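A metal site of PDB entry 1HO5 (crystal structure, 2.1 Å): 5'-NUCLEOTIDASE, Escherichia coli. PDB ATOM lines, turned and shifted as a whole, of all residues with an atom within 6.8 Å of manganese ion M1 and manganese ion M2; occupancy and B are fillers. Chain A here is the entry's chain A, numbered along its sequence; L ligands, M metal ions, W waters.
Merely in contact with manganese ion M2: His 92 (3.9 Å). Of the 19 residues printed, 5 come within 4 Å of manganese ion M2.
OE1 of Gln 229 is bound to manganese ion M1, 1.9 Å away. Manganese ion M1 is bound by OD2 of Asp 59. Manganese ion M1 is bound by OD2 of Asp 16, at 2.1 Å. Manganese ion M1 is bound by a ring nitrogen (NE2) of His 18 (2.2 Å). Water W2 binds manganese ion M1, at 2.2 Å. Water W1 is bound to manganese ion M1 (2.3 Å).
The side-chain amide nitrogen (NE2) of Gln 229 is in hydrogen-bond range of the side-chain carboxylate (OE1) of Glu 265, 2.8 Å away. The side-chain carboxylate of Asp 16 lies within hydrogen-bond range of the side-chain amide nitrogen of Asn 15. A ring nitrogen (ND1) of His 18 is in hydrogen-bond range of the backbone carbonyl oxygen (O) of Asn 61, 2.9 Å away. The backbone NH (N) of Asp 16 sits at hydrogen-bond distance from the backbone carbonyl oxygen (O) of Gly 58 (2.7 Å). The backbone carbonyl oxygen (O) of Asp 59 is in hydrogen-bond range of the backbone NH (N) of His 17, 3.1 Å away. The backbone NH (N) of His 227 lies within hydrogen-bond range of the side-chain carboxylate (OD1) of Asp 16, at 2.8 Å. The backbone carbonyl oxygen (O) of His 192 sits at hydrogen-bond distance from the backbone NH (N) of Thr 147 (2.9 Å). N of His 92 lies within hydrogen-bond range of OD1 of Asp 59 (3.1 Å).
Within 4 Å of manganese ion M1: Asp 16, His 18, Asp 59 and Gln 229.
Manganese ion M2 is bound by OD1 of Asn 91 (2.0 Å), NE2 of His 192 (2.2 Å), O4 of the ligand (2.3 Å), ND1 of His 227 (2.3 Å), OD2 of Asp 59 (2.5 Å) and water W1 (2.6 Å).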
ATOM      1  N   ASN A  15     -27.679   3.224  -1.954  1.00  0.00           N
ATOM      2  CA  ASN A  15     -27.511   3.075  -0.488  1.00  0.00           C
ATOM      3  C   ASN A  15     -28.353   4.155   0.115  1.00  0.00           C
ATOM      4  O   ASN A  15     -28.747   5.111  -0.580  1.00  0.00           O
ATOM      5  CB  ASN A  15     -26.069   3.358  -0.043  1.00  0.00           C
ATOM      6  CG  ASN A  15     -25.585   4.670  -0.580  1.00  0.00           C
ATOM      7  OD1 ASN A  15     -25.323   4.781  -1.760  1.00  0.00           O
ATOM      8  ND2 ASN A  15     -25.539   5.690   0.257  1.00  0.00           N
ATOM      9  N   ASP A  16     -28.614   4.003   1.409  1.00  0.00           N
ATOM     10  CA  ASP A  16     -29.400   4.964   2.183  1.00  0.00           C
ATOM     11  C   ASP A  16     -30.702   5.325   1.490  1.00  0.00           C
ATOM     12  O   ASP A  16     -31.089   6.485   1.307  1.00  0.00           O
ATOM     13  CB  ASP A  16     -28.529   6.168   2.516  1.00  0.00           C
ATOM     14  CG  ASP A  16     -27.351   5.750   3.360  1.00  0.00           C
ATOM     15  OD1 ASP A  16     -26.372   5.217   2.784  1.00  0.00           O
ATOM     16  OD2 ASP A  16     -27.448   5.872   4.599  1.00  0.00           O
ATOM     17  N   HIS A  17     -31.429   4.262   1.186  1.00  0.00           N
ATOM     18  CA  HIS A  17     -32.696   4.414   0.497  1.00  0.00           C
ATOM     19  C   HIS A  17     -33.702   5.217   1.365  1.00  0.00           C
ATOM     20  O   HIS A  17     -34.414   6.108   0.853  1.00  0.00           O
ATOM     21  CB  HIS A  17     -33.236   3.019   0.202  1.00  0.00           C
ATOM     22  CG  HIS A  17     -34.592   3.028  -0.415  1.00  0.00           C
ATOM     23  ND1 HIS A  17     -34.803   3.417  -1.721  1.00  0.00           N
ATOM     24  CD2 HIS A  17     -35.795   2.665   0.084  1.00  0.00           C
ATOM     25  CE1 HIS A  17     -36.093   3.269  -2.014  1.00  0.00           C
ATOM     26  NE2 HIS A  17     -36.711   2.820  -0.944  1.00  0.00           N
ATOM     27  N   HIS A  18     -33.744   4.869   2.647  1.00  0.00           N
ATOM     28  CA  HIS A  18     -34.581   5.520   3.641  1.00  0.00           C
ATOM     29  C   HIS A  18     -36.065   5.705   3.253  1.00  0.00           C
ATOM     30  O   HIS A  18     -36.605   6.819   3.273  1.00  0.00           O
ATOM     31  CB  HIS A  18     -33.931   6.860   4.043  1.00  0.00           C
ATOM     32  CG  HIS A  18     -32.704   6.703   4.910  1.00  0.00           C
ATOM     33  ND1 HIS A  18     -32.744   6.090   6.153  1.00  0.00           N
ATOM     34  CD2 HIS A  18     -31.389   6.980   4.677  1.00  0.00           C
ATOM     35  CE1 HIS A  18     -31.515   6.001   6.645  1.00  0.00           C
ATOM     36  NE2 HIS A  18     -30.683   6.525   5.763  1.00  0.00           N
ATOM     37  N   GLY A  58     -27.259  -0.276   2.262  1.00  0.00           N
ATOM     38  CA  GLY A  58     -28.128  -0.283   3.428  1.00  0.00           C
ATOM     39  C   GLY A  58     -28.858   0.977   3.859  1.00  0.00           C
ATOM     40  O   GLY A  58     -28.878   1.951   3.140  1.00  0.00           O
ATOM     41  N   ASP A  59     -29.434   0.943   5.056  1.00  0.00           N
ATOM     42  CA  ASP A  59     -30.203   2.089   5.581  1.00  0.00           C
ATOM     43  C   ASP A  59     -31.467   2.251   4.693  1.00  0.00           C
ATOM     44  O   ASP A  59     -31.723   3.337   4.133  1.00  0.00           O
ATOM     45  CB  ASP A  59     -29.343   3.391   5.539  1.00  0.00           C
ATOM     46  CG  ASP A  59     -28.835   3.847   6.913  1.00  0.00           C
ATOM     47  OD1 ASP A  59     -28.738   3.010   7.801  1.00  0.00           O
ATOM     48  OD2 ASP A  59     -28.505   5.055   7.068  1.00  0.00           O
ATOM     49  N   ASN A  61     -34.553   1.417   5.889  1.00  0.00           N
ATOM     50  CA  ASN A  61     -35.516   1.878   6.908  1.00  0.00           C
ATOM     51  C   ASN A  61     -35.472   3.345   7.316  1.00  0.00           C
ATOM     52  O   ASN A  61     -34.392   3.960   7.349  1.00  0.00           O
ATOM     53  CB  ASN A  61     -35.355   1.036   8.218  1.00  0.00           C
ATOM     54  CG  ASN A  61     -35.896  -0.373   8.089  1.00  0.00           C
ATOM     55  OD1 ASN A  61     -37.097  -0.603   8.213  1.00  0.00           O
ATOM     56  ND2 ASN A  61     -35.017  -1.327   7.844  1.00  0.00           N
ATOM     57  N   GLY A  90     -27.601  -1.875   7.369  1.00  0.00           N
ATOM     58  CA  GLY A  90     -27.238  -0.545   7.833  1.00  0.00           C
ATOM     59  C   GLY A  90     -27.738  -0.276   9.269  1.00  0.00           C
ATOM     60  O   GLY A  90     -28.635  -0.966   9.774  1.00  0.00           O
ATOM     61  N   ASN A  91     -27.219   0.764   9.903  1.00  0.00           N
ATOM     62  CA  ASN A  91     -27.640   1.006  11.296  1.00  0.00           C
ATOM     63  C   ASN A  91     -29.140   1.249  11.437  1.00  0.00           C
ATOM     64  O   ASN A  91     -29.740   0.804  12.422  1.00  0.00           O
ATOM     65  CB  ASN A  91     -26.862   2.160  11.925  1.00  0.00           C
ATOM     66  CG  ASN A  91     -26.945   3.437  11.121  1.00  0.00           C
ATOM     67  OD1 ASN A  91     -26.627   3.462   9.908  1.00  0.00           O
ATOM     68  ND2 ASN A  91     -27.333   4.512  11.783  1.00  0.00           N
ATOM     69  N   HIS A  92     -29.742   1.956  10.488  1.00  0.00           N
ATOM     70  CA  HIS A  92     -31.181   2.179  10.620  1.00  0.00           C
ATOM     71  C   HIS A  92     -32.003   0.909  10.467  1.00  0.00           C
ATOM     72  O   HIS A  92     -33.189   0.963  10.648  1.00  0.00           O
ATOM     73  CB  HIS A  92     -31.686   3.249   9.665  1.00  0.00           C
ATOM     74  CG  HIS A  92     -31.317   4.613  10.114  1.00  0.00           C
ATOM     75  ND1 HIS A  92     -32.092   5.328  10.990  1.00  0.00           N
ATOM     76  CD2 HIS A  92     -30.180   5.328   9.938  1.00  0.00           C
ATOM     77  CE1 HIS A  92     -31.454   6.427  11.341  1.00  0.00           C
ATOM     78  NE2 HIS A  92     -30.284   6.445  10.717  1.00  0.00           N
ATOM     79  N   THR A 147     -21.440  -0.378  10.266  1.00  0.00           N
ATOM     80  CA  THR A 147     -20.711   0.530  11.184  1.00  0.00           C
ATOM     81  C   THR A 147     -20.912   0.165  12.660  1.00  0.00           C
ATOM     82  O   THR A 147     -22.025  -0.157  13.086  1.00  0.00           O
ATOM     83  CB  THR A 147     -21.148   1.990  11.018  1.00  0.00           C
ATOM     84  OG1 THR A 147     -20.398   2.806  11.933  1.00  0.00           O
ATOM     85  CG2 THR A 147     -22.659   2.175  11.304  1.00  0.00           C
ATOM     86  N   ILE A 153     -25.017   4.980  18.692  1.00  0.00           N
ATOM     87  CA  ILE A 153     -25.930   6.062  18.425  1.00  0.00           C
ATOM     88  C   ILE A 153     -27.397   5.622  18.360  1.00  0.00           C
ATOM     89  O   ILE A 153     -28.301   6.455  18.241  1.00  0.00           O
ATOM     90  CB  ILE A 153     -25.552   6.820  17.123  1.00  0.00           C
ATOM     91  CG1 ILE A 153     -25.597   5.897  15.917  1.00  0.00           C
ATOM     92  CG2 ILE A 153     -24.140   7.423  17.265  1.00  0.00           C
ATOM     93  CD1 ILE A 153     -24.987   6.515  14.693  1.00  0.00           C
ATOM     94  N   HIS A 192     -21.871  -0.370   5.238  1.00  0.00           N
ATOM     95  CA  HIS A 192     -22.660   0.772   5.682  1.00  0.00           C
ATOM     96  C   HIS A 192     -21.722   1.381   6.721  1.00  0.00           C
ATOM     97  O   HIS A 192     -21.958   1.239   7.934  1.00  0.00           O
ATOM     98  CB  HIS A 192     -23.950   0.336   6.381  1.00  0.00           C
ATOM     99  CG  HIS A 192     -24.871   1.493   6.619  1.00  0.00           C
ATOM    100  ND1 HIS A 192     -25.559   2.101   5.583  1.00  0.00           N
ATOM    101  CD2 HIS A 192     -25.048   2.268   7.705  1.00  0.00           C
ATOM    102  CE1 HIS A 192     -26.110   3.218   6.027  1.00  0.00           C
ATOM    103  NE2 HIS A 192     -25.812   3.346   7.313  1.00  0.00           N
ATOM    104  N   GLY A 226     -22.030   3.426   2.020  1.00  0.00           N
ATOM    105  CA  GLY A 226     -23.212   4.165   2.416  1.00  0.00           C
ATOM    106  C   GLY A 226     -22.970   4.871   3.741  1.00  0.00           C
ATOM    107  O   GLY A 226     -21.801   5.163   4.076  1.00  0.00           O
ATOM    108  N   HIS A 227     -24.076   5.241   4.394  1.00  0.00           N
ATOM    109  CA  HIS A 227     -24.092   5.834   5.748  1.00  0.00           C
ATOM    110  C   HIS A 227     -23.770   7.302   5.800  1.00  0.00           C
ATOM    111  O   HIS A 227     -24.559   8.096   6.314  1.00  0.00           O
ATOM    112  CB  HIS A 227     -23.109   5.006   6.668  1.00  0.00           C
ATOM    113  CG  HIS A 227     -23.134   5.394   8.128  1.00  0.00           C
ATOM    114  ND1 HIS A 227     -24.308   5.551   8.843  1.00  0.00           N
ATOM    115  CD2 HIS A 227     -22.122   5.591   9.011  1.00  0.00           C
ATOM    116  CE1 HIS A 227     -24.019   5.816  10.109  1.00  0.00           C
ATOM    117  NE2 HIS A 227     -22.694   5.856  10.232  1.00  0.00           N
ATOM    118  N   SER A 228     -22.658   7.695   5.196  1.00  0.00           N
ATOM    119  CA  SER A 228     -22.289   9.086   5.219  1.00  0.00           C
ATOM    120  C   SER A 228     -23.201   9.857   4.304  1.00  0.00           C
ATOM    121  O   SER A 228     -23.384  11.076   4.434  1.00  0.00           O
ATOM    122  CB  SER A 228     -20.818   9.274   4.813  1.00  0.00           C
ATOM    123  OG  SER A 228     -20.466   8.585   3.622  1.00  0.00           O
ATOM    124  N   GLN A 229     -23.816   9.129   3.378  1.00  0.00           N
ATOM    125  CA  GLN A 229     -24.731   9.730   2.414  1.00  0.00           C
ATOM    126  C   GLN A 229     -24.093  10.800   1.546  1.00  0.00           C
ATOM    127  O   GLN A 229     -24.376  11.991   1.613  1.00  0.00           O
ATOM    128  CB  GLN A 229     -26.012  10.210   3.109  1.00  0.00           C
ATOM    129  CG  GLN A 229     -26.719   9.002   3.825  1.00  0.00           C
ATOM    130  CD  GLN A 229     -28.150   9.274   4.372  1.00  0.00           C
ATOM    131  OE1 GLN A 229     -28.664   8.519   5.235  1.00  0.00           O
ATOM    132  NE2 GLN A 229     -28.793  10.325   3.868  1.00  0.00           N
ATOM    133  N   GLU A 265     -27.930   9.122  -1.748  1.00  0.00           N
ATOM    134  CA  GLU A 265     -29.039   8.712  -0.918  1.00  0.00           C
ATOM    135  C   GLU A 265     -30.348   8.605  -1.684  1.00  0.00           C
ATOM    136  O   GLU A 265     -30.460   9.040  -2.826  1.00  0.00           O
ATOM    137  CB  GLU A 265     -29.235   9.761   0.196  1.00  0.00           C
ATOM    138  CG  GLU A 265     -29.689  11.118  -0.356  1.00  0.00           C
ATOM    139  CD  GLU A 265     -29.440  12.303   0.586  1.00  0.00           C
ATOM    140  OE1 GLU A 265     -28.884  12.112   1.708  1.00  0.00           O
ATOM    141  OE2 GLU A 265     -29.823  13.422   0.203  1.00  0.00           O
ATOM    142  N   ARG A 350     -30.610  19.043   9.702  1.00  0.00           N
ATOM    143  CA  ARG A 350     -29.496  18.532  10.493  1.00  0.00           C
ATOM    144  C   ARG A 350     -28.415  19.592  10.730  1.00  0.00           C
ATOM    145  O   ARG A 350     -28.005  19.836  11.869  1.00  0.00           O
ATOM    146  CB  ARG A 350     -28.888  17.296   9.813  1.00  0.00           C
ATOM    147  CG  ARG A 350     -28.273  16.298  10.781  1.00  0.00           C
ATOM    148  CD  ARG A 350     -27.000  15.694  10.223  1.00  0.00           C
ATOM    149  NE  ARG A 350     -27.095  14.247  10.004  1.00  0.00           N
ATOM    150  CZ  ARG A 350     -26.045  13.462   9.764  1.00  0.00           C
ATOM    151  NH1 ARG A 350     -24.826  13.984   9.708  1.00  0.00           N
ATOM    152  NH2 ARG A 350     -26.215  12.161   9.567  1.00  0.00           N
HETATM  153  P1  LIG L   1     -27.078   7.861  10.464  1.00  0.00           P
HETATM  154  O1  LIG L   1     -28.335   8.332  11.116  1.00  0.00           O
HETATM  155  O2  LIG L   1     -26.864   8.645   9.180  1.00  0.00           O
HETATM  156  O3  LIG L   1     -25.934   8.114  11.376  1.00  0.00           O
HETATM  157  O4  LIG L   1     -27.185   6.410  10.181  1.00  0.00           O
HETATM  158 MN    MN M   1     -28.544   6.820   6.168  1.00  0.00          MN
HETATM  159 MN    MN M   2     -26.526   4.970   8.544  1.00  0.00          MN
HETATM  160  O   HOH W   1     -26.611   7.262   7.360  1.00  0.00           O
HETATM  161  O   HOH W   2     -29.297   7.833   8.000  1.00  0.00           O
